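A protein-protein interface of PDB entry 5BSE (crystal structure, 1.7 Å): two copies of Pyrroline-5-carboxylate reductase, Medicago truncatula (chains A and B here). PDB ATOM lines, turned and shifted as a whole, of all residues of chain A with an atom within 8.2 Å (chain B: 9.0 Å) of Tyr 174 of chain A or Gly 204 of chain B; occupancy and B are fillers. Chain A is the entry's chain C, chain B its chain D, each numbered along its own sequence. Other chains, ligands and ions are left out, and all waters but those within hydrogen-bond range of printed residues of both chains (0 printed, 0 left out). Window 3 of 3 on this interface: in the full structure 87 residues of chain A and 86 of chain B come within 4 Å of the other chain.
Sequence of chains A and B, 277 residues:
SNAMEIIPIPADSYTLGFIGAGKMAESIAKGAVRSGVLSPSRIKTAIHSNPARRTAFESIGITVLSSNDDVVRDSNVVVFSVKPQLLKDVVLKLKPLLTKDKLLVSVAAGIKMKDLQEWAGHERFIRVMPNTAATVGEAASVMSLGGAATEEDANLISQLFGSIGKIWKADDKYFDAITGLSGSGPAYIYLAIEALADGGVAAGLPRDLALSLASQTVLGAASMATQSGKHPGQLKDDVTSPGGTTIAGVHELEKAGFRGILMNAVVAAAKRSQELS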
ATOM      1  N   ARG A 127     -21.389  17.107 -36.979  1.00  0.00           N
ATOM      2  CA  ARG A 127     -21.660  17.960 -35.829  1.00  0.00           C
ATOM      3  C   ARG A 127     -20.987  19.285 -36.106  1.00  0.00           C
ATOM      4  O   ARG A 127     -19.833  19.342 -36.562  1.00  0.00           O
ATOM      5  CB  ARG A 127     -21.108  17.369 -34.549  1.00  0.00           C
ATOM      6  CG  ARG A 127     -21.236  18.261 -33.344  1.00  0.00           C
ATOM      7  CD  ARG A 127     -20.525  17.675 -32.172  1.00  0.00           C
ATOM      8  NE  ARG A 127     -20.668  18.524 -30.995  1.00  0.00           N
ATOM      9  CZ  ARG A 127     -20.024  18.281 -29.871  1.00  0.00           C
ATOM     10  NH1 ARG A 127     -19.261  17.239 -29.753  1.00  0.00           N
ATOM     11  NH2 ARG A 127     -20.135  19.111 -28.856  1.00  0.00           N
ATOM     12  N   MET A 129     -20.398  23.179 -34.220  1.00  0.00           N
ATOM     13  CA  MET A 129     -20.537  24.059 -33.079  1.00  0.00           C
ATOM     14  C   MET A 129     -20.276  25.481 -33.574  1.00  0.00           C
ATOM     15  O   MET A 129     -19.137  25.869 -33.748  1.00  0.00           O
ATOM     16  CB  MET A 129     -19.544  23.740 -31.973  1.00  0.00           C
ATOM     17  CG  MET A 129     -19.528  24.750 -30.818  1.00  0.00           C
ATOM     18  SD  MET A 129     -21.032  24.740 -29.901  1.00  0.00           S
ATOM     19  CE  MET A 129     -20.778  26.012 -28.576  1.00  0.00           C
ATOM     20  N   VAL A 142     -16.936  25.154 -35.804  1.00  0.00           N
ATOM     21  CA  VAL A 142     -16.097  23.997 -36.064  1.00  0.00           C
ATOM     22  C   VAL A 142     -16.975  22.781 -36.352  1.00  0.00           C
ATOM     23  O   VAL A 142     -18.031  22.635 -35.769  1.00  0.00           O
ATOM     24  CB  VAL A 142     -15.231  23.698 -34.872  1.00  0.00           C
ATOM     25  CG1 VAL A 142     -14.257  22.595 -35.199  1.00  0.00           C
ATOM     26  CG2 VAL A 142     -14.348  24.895 -34.509  1.00  0.00           C
ATOM     27  N   SER A 144     -17.208  18.433 -36.973  1.00  0.00           N
ATOM     28  CA  SER A 144     -16.615  17.107 -36.818  1.00  0.00           C
ATOM     29  C   SER A 144     -17.482  16.128 -37.585  1.00  0.00           C
ATOM     30  O   SER A 144     -18.664  16.320 -37.783  1.00  0.00           O
ATOM     31  CB  SER A 144     -16.491  16.638 -35.367  1.00  0.00           C
ATOM     32  OG  SER A 144     -17.778  16.532 -34.813  1.00  0.00           O
ATOM     33  N   LYS A 169     -12.441  22.416 -39.374  1.00  0.00           N
ATOM     34  CA  LYS A 169     -12.677  21.045 -39.030  1.00  0.00           C
ATOM     35  C   LYS A 169     -11.895  20.722 -37.803  1.00  0.00           C
ATOM     36  O   LYS A 169     -10.770  21.163 -37.612  1.00  0.00           O
ATOM     37  CB  LYS A 169     -12.260  20.126 -40.175  1.00  0.00           C
ATOM     38  CG  LYS A 169     -13.210  20.368 -41.329  1.00  0.00           C
ATOM     39  CD  LYS A 169     -12.942  19.520 -42.562  1.00  0.00           C
ATOM     40  CE  LYS A 169     -13.705  20.134 -43.732  1.00  0.00           C
ATOM     41  NZ  LYS A 169     -13.464  19.349 -44.956  1.00  0.00           N
ATOM     42  N   ALA A 170     -12.483  19.947 -36.933  1.00  0.00           N
ATOM     43  CA  ALA A 170     -11.762  19.451 -35.775  1.00  0.00           C
ATOM     44  C   ALA A 170     -12.365  18.175 -35.273  1.00  0.00           C
ATOM     45  O   ALA A 170     -13.533  17.919 -35.415  1.00  0.00           O
ATOM     46  CB  ALA A 170     -11.771  20.451 -34.648  1.00  0.00           C
ATOM     47  N   ASP A 171     -11.503  17.387 -34.626  1.00  0.00           N
ATOM     48  CA  ASP A 171     -11.896  16.137 -34.038  1.00  0.00           C
ATOM     49  C   ASP A 171     -12.918  16.426 -32.940  1.00  0.00           C
ATOM     50  O   ASP A 171     -12.811  17.413 -32.191  1.00  0.00           O
ATOM     51  CB  ASP A 171     -10.670  15.458 -33.444  1.00  0.00           C
ATOM     52  CG  ASP A 171      -9.783  14.793 -34.494  1.00  0.00           C
ATOM     53  OD1 ASP A 171     -10.088  14.810 -35.715  1.00  0.00           O
ATOM     54  OD2 ASP A 171      -8.802  14.180 -34.082  1.00  0.00           O
ATOM     55  N   ASP A 172     -13.881  15.532 -32.816  1.00  0.00           N
ATOM     56  CA  ASP A 172     -14.961  15.691 -31.840  1.00  0.00           C
ATOM     57  C   ASP A 172     -14.394  15.815 -30.440  1.00  0.00           C
ATOM     58  O   ASP A 172     -14.988  16.535 -29.611  1.00  0.00           O
ATOM     59  CB  ASP A 172     -15.925  14.497 -31.941  1.00  0.00           C
ATOM     60  CG  ASP A 172     -17.342  14.857 -31.509  1.00  0.00           C
ATOM     61  OD1 ASP A 172     -17.944  15.773 -32.096  1.00  0.00           O
ATOM     62  OD2 ASP A 172     -17.855  14.271 -30.558  1.00  0.00           O
ATOM     63  N   LYS A 173     -13.236  15.262 -30.165  1.00  0.00           N
ATOM     64  CA  LYS A 173     -12.703  15.332 -28.810  1.00  0.00           C
ATOM     65  C   LYS A 173     -12.354  16.757 -28.342  1.00  0.00           C
ATOM     66  O   LYS A 173     -12.177  16.972 -27.183  1.00  0.00           O
ATOM     67  CB  LYS A 173     -11.474  14.465 -28.639  1.00  0.00           C
ATOM     68  CG  LYS A 173     -10.267  14.976 -29.344  1.00  0.00           C
ATOM     69  CD  LYS A 173      -9.166  13.958 -29.258  1.00  0.00           C
ATOM     70  CE  LYS A 173      -8.030  14.459 -30.079  1.00  0.00           C
ATOM     71  NZ  LYS A 173      -6.999  13.389 -30.135  1.00  0.00           N
ATOM     72  N   TYR A 174     -12.209  17.661 -29.305  1.00  0.00           N
ATOM     73  CA  TYR A 174     -11.808  19.055 -29.004  1.00  0.00           C
ATOM     74  C   TYR A 174     -13.000  19.917 -28.661  1.00  0.00           C
ATOM     75  O   TYR A 174     -12.798  21.089 -28.321  1.00  0.00           O
ATOM     76  CB  TYR A 174     -11.048  19.639 -30.153  1.00  0.00           C
ATOM     77  CG  TYR A 174      -9.716  18.974 -30.440  1.00  0.00           C
ATOM     78  CD1 TYR A 174      -8.776  18.832 -29.448  1.00  0.00           C
ATOM     79  CD2 TYR A 174      -9.411  18.522 -31.686  1.00  0.00           C
ATOM     80  CE1 TYR A 174      -7.552  18.241 -29.726  1.00  0.00           C
ATOM     81  CE2 TYR A 174      -8.195  17.935 -31.985  1.00  0.00           C
ATOM     82  CZ  TYR A 174      -7.294  17.772 -30.990  1.00  0.00           C
ATOM     83  OH  TYR A 174      -6.094  17.195 -31.259  1.00  0.00           O
ATOM     84  N   PHE A 175     -14.208  19.405 -28.775  1.00  0.00           N
ATOM     85  CA  PHE A 175     -15.375  20.277 -28.765  1.00  0.00           C
ATOM     86  C   PHE A 175     -15.622  20.902 -27.374  1.00  0.00           C
ATOM     87  O   PHE A 175     -16.078  22.094 -27.289  1.00  0.00           O
ATOM     88  CB  PHE A 175     -16.593  19.591 -29.358  1.00  0.00           C
ATOM     89  CG  PHE A 175     -16.694  19.737 -30.829  1.00  0.00           C
ATOM     90  CD1 PHE A 175     -15.704  19.304 -31.650  1.00  0.00           C
ATOM     91  CD2 PHE A 175     -17.758  20.370 -31.391  1.00  0.00           C
ATOM     92  CE1 PHE A 175     -15.778  19.492 -33.006  1.00  0.00           C
ATOM     93  CE2 PHE A 175     -17.846  20.516 -32.733  1.00  0.00           C
ATOM     94  CZ  PHE A 175     -16.850  20.110 -33.545  1.00  0.00           C
ATOM     95  N   ASP A 176     -15.256  20.260 -26.271  1.00  0.00           N
ATOM     96  CA  ASP A 176     -15.256  21.058 -24.947  1.00  0.00           C
ATOM     97  C   ASP A 176     -14.389  22.251 -24.849  1.00  0.00           C
ATOM     98  O   ASP A 176     -14.800  23.338 -24.419  1.00  0.00           O
ATOM     99  CB  ASP A 176     -14.895  20.173 -23.778  1.00  0.00           C
ATOM    100  CG  ASP A 176     -15.928  19.124 -23.524  1.00  0.00           C
ATOM    101  OD1 ASP A 176     -17.119  19.425 -23.635  1.00  0.00           O
ATOM    102  OD2 ASP A 176     -15.496  17.997 -23.161  1.00  0.00           O
ATOM    103  N   ALA A 177     -13.177  22.135 -25.275  1.00  0.00           N
ATOM    104  CA  ALA A 177     -12.308  23.254 -25.317  1.00  0.00           C
ATOM    105  C   ALA A 177     -12.817  24.346 -26.293  1.00  0.00           C
ATOM    106  O   ALA A 177     -12.614  25.540 -26.106  1.00  0.00           O
ATOM    107  CB  ALA A 177     -10.902  22.807 -25.693  1.00  0.00           C
ATOM    108  N   ILE A 178     -13.302  23.900 -27.443  1.00  0.00           N
ATOM    109  CA  ILE A 178     -13.738  24.840 -28.403  1.00  0.00           C
ATOM    110  C   ILE A 178     -14.853  25.636 -27.756  1.00  0.00           C
ATOM    111  O   ILE A 178     -14.944  26.864 -27.935  1.00  0.00           O
ATOM    112  CB  ILE A 178     -14.196  24.150 -29.668  1.00  0.00           C
ATOM    113  CG1 ILE A 178     -12.987  23.558 -30.413  1.00  0.00           C
ATOM    114  CG2 ILE A 178     -14.967  25.096 -30.578  1.00  0.00           C
ATOM    115  CD1 ILE A 178     -13.325  22.499 -31.456  1.00  0.00           C
ATOM    116  N   THR A 179     -15.704  24.950 -27.019  1.00  0.00           N
ATOM    117  CA  THR A 179     -16.849  25.602 -26.382  1.00  0.00           C
ATOM    118  C   THR A 179     -16.376  26.739 -25.458  1.00  0.00           C
ATOM    119  O   THR A 179     -16.941  27.821 -25.453  1.00  0.00           O
ATOM    120  CB  THR A 179     -17.703  24.568 -25.660  1.00  0.00           C
ATOM    121  OG1 THR A 179     -18.208  23.628 -26.648  1.00  0.00           O
ATOM    122  CG2 THR A 179     -18.854  25.240 -25.005  1.00  0.00           C
ATOM    123  N   GLY A 180     -15.272  26.496 -24.752  1.00  0.00           N
ATOM    124  CA  GLY A 180     -14.737  27.480 -23.877  1.00  0.00           C
ATOM    125  C   GLY A 180     -14.113  28.687 -24.533  1.00  0.00           C
ATOM    126  O   GLY A 180     -13.918  29.736 -23.915  1.00  0.00           O
ATOM    127  N   LEU A 181     -13.668  28.511 -25.770  1.00  0.00           N
ATOM    128  CA  LEU A 181     -12.987  29.529 -26.531  1.00  0.00           C
ATOM    129  C   LEU A 181     -13.982  30.243 -27.470  1.00  0.00           C
ATOM    130  O   LEU A 181     -14.342  31.356 -27.267  1.00  0.00           O
ATOM    131  CB  LEU A 181     -11.823  28.886 -27.257  1.00  0.00           C
ATOM    132  CG  LEU A 181     -11.084  29.840 -28.220  1.00  0.00           C
ATOM    133  CD1 LEU A 181     -10.661  31.120 -27.523  1.00  0.00           C
ATOM    134  CD2 LEU A 181      -9.863  29.133 -28.740  1.00  0.00           C
ATOM    135  N   SER A 182     -14.449  29.562 -28.506  1.00  0.00           N
ATOM    136  CA  SER A 182     -15.366  30.254 -29.460  1.00  0.00           C
ATOM    137  C   SER A 182     -16.778  30.305 -29.031  1.00  0.00           C
ATOM    138  O   SER A 182     -17.457  31.220 -29.405  1.00  0.00           O
ATOM    139  CB  SER A 182     -15.206  29.627 -30.881  1.00  0.00           C
ATOM    140  OG  SER A 182     -15.456  28.258 -30.812  1.00  0.00           O
ATOM    141  N   VAL A 266     -10.907  30.775 -20.442  1.00  0.00           N
ATOM    142  CA  VAL A 266     -11.042  29.706 -21.410  1.00  0.00           C
ATOM    143  C   VAL A 266     -10.963  28.381 -20.721  1.00  0.00           C
ATOM    144  O   VAL A 266     -11.791  27.442 -20.958  1.00  0.00           O
ATOM    145  CB  VAL A 266      -9.987  29.773 -22.517  1.00  0.00           C
ATOM    146  CG1 VAL A 266     -10.125  28.568 -23.454  1.00  0.00           C
ATOM    147  CG2 VAL A 266     -10.166  31.067 -23.282  1.00  0.00           C
ATOM    148  N   VAL A 267      -9.939  28.157 -19.890  1.00  0.00           N
ATOM    149  CA  VAL A 267      -9.799  26.913 -19.181  1.00  0.00           C
ATOM    150  C   VAL A 267     -11.050  26.578 -18.304  1.00  0.00           C
ATOM    151  O   VAL A 267     -11.504  25.412 -18.253  1.00  0.00           O
ATOM    152  CB  VAL A 267      -8.492  26.880 -18.362  1.00  0.00           C
ATOM    153  CG1 VAL A 267      -8.456  25.699 -17.428  1.00  0.00           C
ATOM    154  CG2 VAL A 267      -7.344  26.809 -19.391  1.00  0.00           C
ATOM    155  N   ALA A 270     -14.006  25.672 -20.549  1.00  0.00           N
ATOM    156  CA  ALA A 270     -13.800  24.296 -21.057  1.00  0.00           C
ATOM    157  C   ALA A 270     -13.995  23.193 -20.055  1.00  0.00           C
ATOM    158  O   ALA A 270     -14.621  22.164 -20.355  1.00  0.00           O
ATOM    159  CB  ALA A 270     -12.400  24.152 -21.684  1.00  0.00           C
ATOM    160  N   SER A 273     -17.668  22.842 -19.556  1.00  0.00           N
ATOM    161  CA  SER A 273     -18.249  22.145 -20.695  1.00  0.00           C
ATOM    162  C   SER A 273     -18.113  20.655 -20.479  1.00  0.00           C
ATOM    163  O   SER A 273     -19.035  19.891 -20.730  1.00  0.00           O
ATOM    164  CB  SER A 273     -17.527  22.576 -21.962  1.00  0.00           C
ATOM    165  OG  SER A 273     -18.027  21.910 -23.116  1.00  0.00           O
ATOM    166  N   ALA B 197      -5.922  32.308 -27.434  1.00  0.00           N
ATOM    167  CA  ALA B 197      -5.358  31.149 -28.108  1.00  0.00           C
ATOM    168  C   ALA B 197      -4.525  30.272 -27.163  1.00  0.00           C
ATOM    169  O   ALA B 197      -4.675  29.057 -27.169  1.00  0.00           O
ATOM    170  CB  ALA B 197      -4.480  31.654 -29.275  1.00  0.00           C
ATOM    171  N   ASP B 198      -3.710  30.885 -26.344  1.00  0.00           N
ATOM    172  CA  ASP B 198      -2.983  30.177 -25.357  1.00  0.00           C
ATOM    173  C   ASP B 198      -3.898  29.436 -24.389  1.00  0.00           C
ATOM    174  O   ASP B 198      -3.616  28.303 -23.996  1.00  0.00           O
ATOM    175  CB  ASP B 198      -2.062  31.124 -24.537  1.00  0.00           C
ATOM    176  CG  ASP B 198      -0.783  31.585 -25.254  1.00  0.00           C
ATOM    177  OD1 ASP B 198      -0.338  30.900 -26.235  1.00  0.00           O
ATOM    178  OD2 ASP B 198      -0.270  32.690 -24.886  1.00  0.00           O
ATOM    179  N   GLY B 199      -5.049  30.050 -24.049  1.00  0.00           N
ATOM    180  CA  GLY B 199      -6.006  29.402 -23.223  1.00  0.00           C
ATOM    181  C   GLY B 199      -6.608  28.164 -23.885  1.00  0.00           C
ATOM    182  O   GLY B 199      -6.761  27.117 -23.300  1.00  0.00           O
ATOM    183  N   GLY B 200      -6.859  28.297 -25.173  1.00  0.00           N
ATOM    184  CA  GLY B 200      -7.347  27.150 -25.989  1.00  0.00           C
ATOM    185  C   GLY B 200      -6.376  26.010 -26.010  1.00  0.00           C
ATOM    186  O   GLY B 200      -6.726  24.854 -25.736  1.00  0.00           O
ATOM    187  N   VAL B 201      -5.118  26.344 -26.226  1.00  0.00           N
ATOM    188  CA  VAL B 201      -4.054  25.370 -26.147  1.00  0.00           C
ATOM    189  C   VAL B 201      -3.941  24.718 -24.775  1.00  0.00           C
ATOM    190  O   VAL B 201      -3.811  23.497 -24.639  1.00  0.00           O
ATOM    191  CB  VAL B 201      -2.727  25.979 -26.672  1.00  0.00           C
ATOM    192  CG1 VAL B 201      -1.598  24.962 -26.527  1.00  0.00           C
ATOM    193  CG2 VAL B 201      -2.881  26.322 -28.100  1.00  0.00           C
ATOM    194  N   ALA B 202      -4.054  25.521 -23.724  1.00  0.00           N
ATOM    195  CA  ALA B 202      -4.017  25.053 -22.373  1.00  0.00           C
ATOM    196  C   ALA B 202      -5.134  24.092 -22.136  1.00  0.00           C
ATOM    197  O   ALA B 202      -4.954  23.135 -21.380  1.00  0.00           O
ATOM    198  CB  ALA B 202      -3.999  26.204 -21.384  1.00  0.00           C
ATOM    199  N   ALA B 203      -6.277  24.278 -22.800  1.00  0.00           N
ATOM    200  CA  ALA B 203      -7.419  23.404 -22.717  1.00  0.00           C
ATOM    201  C   ALA B 203      -7.377  22.236 -23.658  1.00  0.00           C
ATOM    202  O   ALA B 203      -8.337  21.460 -23.732  1.00  0.00           O
ATOM    203  CB  ALA B 203      -8.676  24.201 -22.874  1.00  0.00           C
ATOM    204  N   GLY B 204      -6.308  22.087 -24.409  1.00  0.00           N
ATOM    205  CA  GLY B 204      -6.108  20.934 -25.266  1.00  0.00           C
ATOM    206  C   GLY B 204      -6.325  21.143 -26.754  1.00  0.00           C
ATOM    207  O   GLY B 204      -6.204  20.188 -27.510  1.00  0.00           O
ATOM    208  N   LEU B 205      -6.593  22.343 -27.206  1.00  0.00           N
ATOM    209  CA  LEU B 205      -6.745  22.606 -28.617  1.00  0.00           C
ATOM    210  C   LEU B 205      -5.448  22.720 -29.382  1.00  0.00           C
ATOM    211  O   LEU B 205      -4.443  23.283 -28.905  1.00  0.00           O
ATOM    212  CB  LEU B 205      -7.482  23.896 -28.854  1.00  0.00           C
ATOM    213  CG  LEU B 205      -8.862  23.990 -28.357  1.00  0.00           C
ATOM    214  CD1 LEU B 205      -9.422  25.333 -28.810  1.00  0.00           C
ATOM    215  CD2 LEU B 205      -9.648  22.814 -28.994  1.00  0.00           C
ATOM    216  N   PRO B 206      -5.454  22.272 -30.631  1.00  0.00           N
ATOM    217  CA  PRO B 206      -4.274  22.525 -31.513  1.00  0.00           C
ATOM    218  C   PRO B 206      -4.072  24.032 -31.651  1.00  0.00           C
ATOM    219  O   PRO B 206      -5.060  24.802 -31.667  1.00  0.00           O
ATOM    220  CB  PRO B 206      -4.709  21.922 -32.862  1.00  0.00           C
ATOM    221  CG  PRO B 206      -5.693  20.860 -32.488  1.00  0.00           C
ATOM    222  CD  PRO B 206      -6.491  21.465 -31.305  1.00  0.00           C
ATOM    223  N   ARG B 207      -2.859  24.431 -31.778  1.00  0.00           N
ATOM    224  CA  ARG B 207      -2.525  25.859 -31.810  1.00  0.00           C
ATOM    225  C   ARG B 207      -3.118  26.579 -32.966  1.00  0.00           C
ATOM    226  O   ARG B 207      -3.639  27.687 -32.848  1.00  0.00           O
ATOM    227  CB  ARG B 207      -0.999  26.009 -31.849  1.00  0.00           C
ATOM    228  CG  ARG B 207      -0.470  27.382 -32.149  1.00  0.00           C
ATOM    229  CD  ARG B 207      -0.809  28.408 -31.076  1.00  0.00           C
ATOM    230  NE  ARG B 207      -0.177  28.081 -29.794  1.00  0.00           N
ATOM    231  CZ  ARG B 207      -0.350  28.797 -28.677  1.00  0.00           C
ATOM    232  NH1 ARG B 207      -1.066  29.915 -28.747  1.00  0.00           N
ATOM    233  NH2 ARG B 207       0.275  28.439 -27.575  1.00  0.00           N
ATOM    234  N   LEU B 209      -5.794  25.976 -34.762  1.00  0.00           N
ATOM    235  CA  LEU B 209      -7.229  26.115 -34.537  1.00  0.00           C
ATOM    236  C   LEU B 209      -7.497  27.170 -33.456  1.00  0.00           C
ATOM    237  O   LEU B 209      -8.377  27.964 -33.540  1.00  0.00           O
ATOM    238  CB  LEU B 209      -7.876  24.816 -34.132  1.00  0.00           C
ATOM    239  CG  LEU B 209      -9.377  24.818 -33.884  1.00  0.00           C
ATOM    240  CD1 LEU B 209     -10.130  25.147 -35.165  1.00  0.00           C
ATOM    241  CD2 LEU B 209      -9.824  23.441 -33.341  1.00  0.00           C
ATOM    242  N   ALA B 210      -6.727  27.065 -32.381  1.00  0.00           N
ATOM    243  CA  ALA B 210      -6.944  27.990 -31.256  1.00  0.00           C
ATOM    244  C   ALA B 210      -6.783  29.403 -31.691  1.00  0.00           C
ATOM    245  O   ALA B 210      -7.577  30.257 -31.320  1.00  0.00           O
ATOM    246  CB  ALA B 210      -6.025  27.666 -30.117  1.00  0.00           C
ATOM    247  N   LEU B 213      -9.641  30.391 -34.084  1.00  0.00           N
ATOM    248  CA  LEU B 213     -10.858  30.612 -33.317  1.00  0.00           C
ATOM    249  C   LEU B 213     -10.819  31.879 -32.531  1.00  0.00           C
ATOM    250  O   LEU B 213     -11.800  32.596 -32.399  1.00  0.00           O
ATOM    251  CB  LEU B 213     -11.168  29.433 -32.413  1.00  0.00           C
ATOM    252  CG  LEU B 213     -11.585  28.139 -33.109  1.00  0.00           C
ATOM    253  CD1 LEU B 213     -11.760  27.075 -32.055  1.00  0.00           C
ATOM    254  CD2 LEU B 213     -12.854  28.298 -33.909  1.00  0.00           C
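The backbone NH (N) of Leu 205 of chain B lies within hydrogen-bond range of the backbone carbonyl oxygen (O) of Gly 200 of chain B (2.9 Å). The backbone carbonyl oxygen (O) of Val 142 of chain A lies within hydrogen-bond range of the backbone NH (N) of Met 129 of chain A (2.9 Å). O of Ile 178 of chain A sits close to OG of Ser 182 of chain A (3.2 Å).
Asp 172 of chain A touches none of the printed residues of chain B. No residue of chain B comes within 4 Å of Lys 173 of chain A. Of chain B, only Gly 204, Leu 205 and Pro 206 come within 4 Å of Tyr 174 of chain A. Of the printed residues of chain B, Ala 177 of chain A touches Ala 203 and Leu 205. Printed residues of chain B within 4 Å of Ile 178 of chain A: Leu 205 (3.7 Å). Of the printed residues of chain A, Ala 202 of chain B touches Val 267. Of chain A, only Ala 177 (3.5 Å) and Ala 270 (3.9 Å) come within 4 Å of Ala 203 of chain B. Of chain A, only Tyr 174 (3.2 Å) comes within 4 Å of Gly 204 of chain B. Printed residues of chain A within 4 Å of Leu 205 of chain B: Tyr 174 (3.7 Å), Ala 177 (3.5 Å), Ile 178 (3.7 Å) and Leu 181 (3.8 Å). Of the printed residues of chain A, Pro 206 of chain B touches Tyr 174. The nearest residue of chain A that does not touch Gly 204 of chain B is Ala 177 of chain A (4.8 Å). The nearest printed residue of chain B that does not touch Ala 170 of chain A is Pro 206 of chain B (6.3 Å).
Printed residues of chain B that touch a printed residue of chain A: Gly 199, Gly 200, Ala 202, Ala 203, Gly 204, Leu 205, Pro 206, Leu 209, Ala 210 and Leu 213. Hydrophobic or aromatic side chains of chain B within 4 Å of the printed part of chain A: Ala 202, Ala 203, Leu 205, Pro 206, Leu 209 and Leu 213. Of the 22 printed residues of chain A, 9 touch a printed residue of chain B. Hydrophobic or aromatic side chains of chain A within 4 Å of the printed part of chain B: Val 142, Ala 170, Tyr 174, Ala 177, Ile 178, Leu 181, Val 266, Val 267 and Ala 270. Along chain A the printed residues that touch a printed residue of chain B span positions 142 to 270.
No position is printed for both chains. Of the 16 pairs that touch across the chains among the printed residues, none has its exchanged pair printed and touching as well.
Leu 213 of chain B touches Val 142 of chain A. CD2 of Leu 209 of chain B touches CB of Ala 170 of chain A, at 3.8 Å. Tyr 174 of chain A touches Gly 204 of chain B. Tyr 174 of chain A touches Leu 205 of chain B (O to CD2, 3.7 Å). Leu 205 of chain B touches Ile 178 of chain A (CD2 to CG1, 3.7 Å). Leu 181 of chain A touches Ala 210 of chain B. CB of Leu 213 of chain B touches CD2 of Leu 181 of chain A (3.9 Å). Val 266 of chain A touches Gly 199 of chain B. Gly 200 of chain B touches Val 266 of chain A (N to CG1, 3.7 Å). Val 267 of chain A touches Ala 202 of chain B (CG2 to CB, 3.9 Å).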
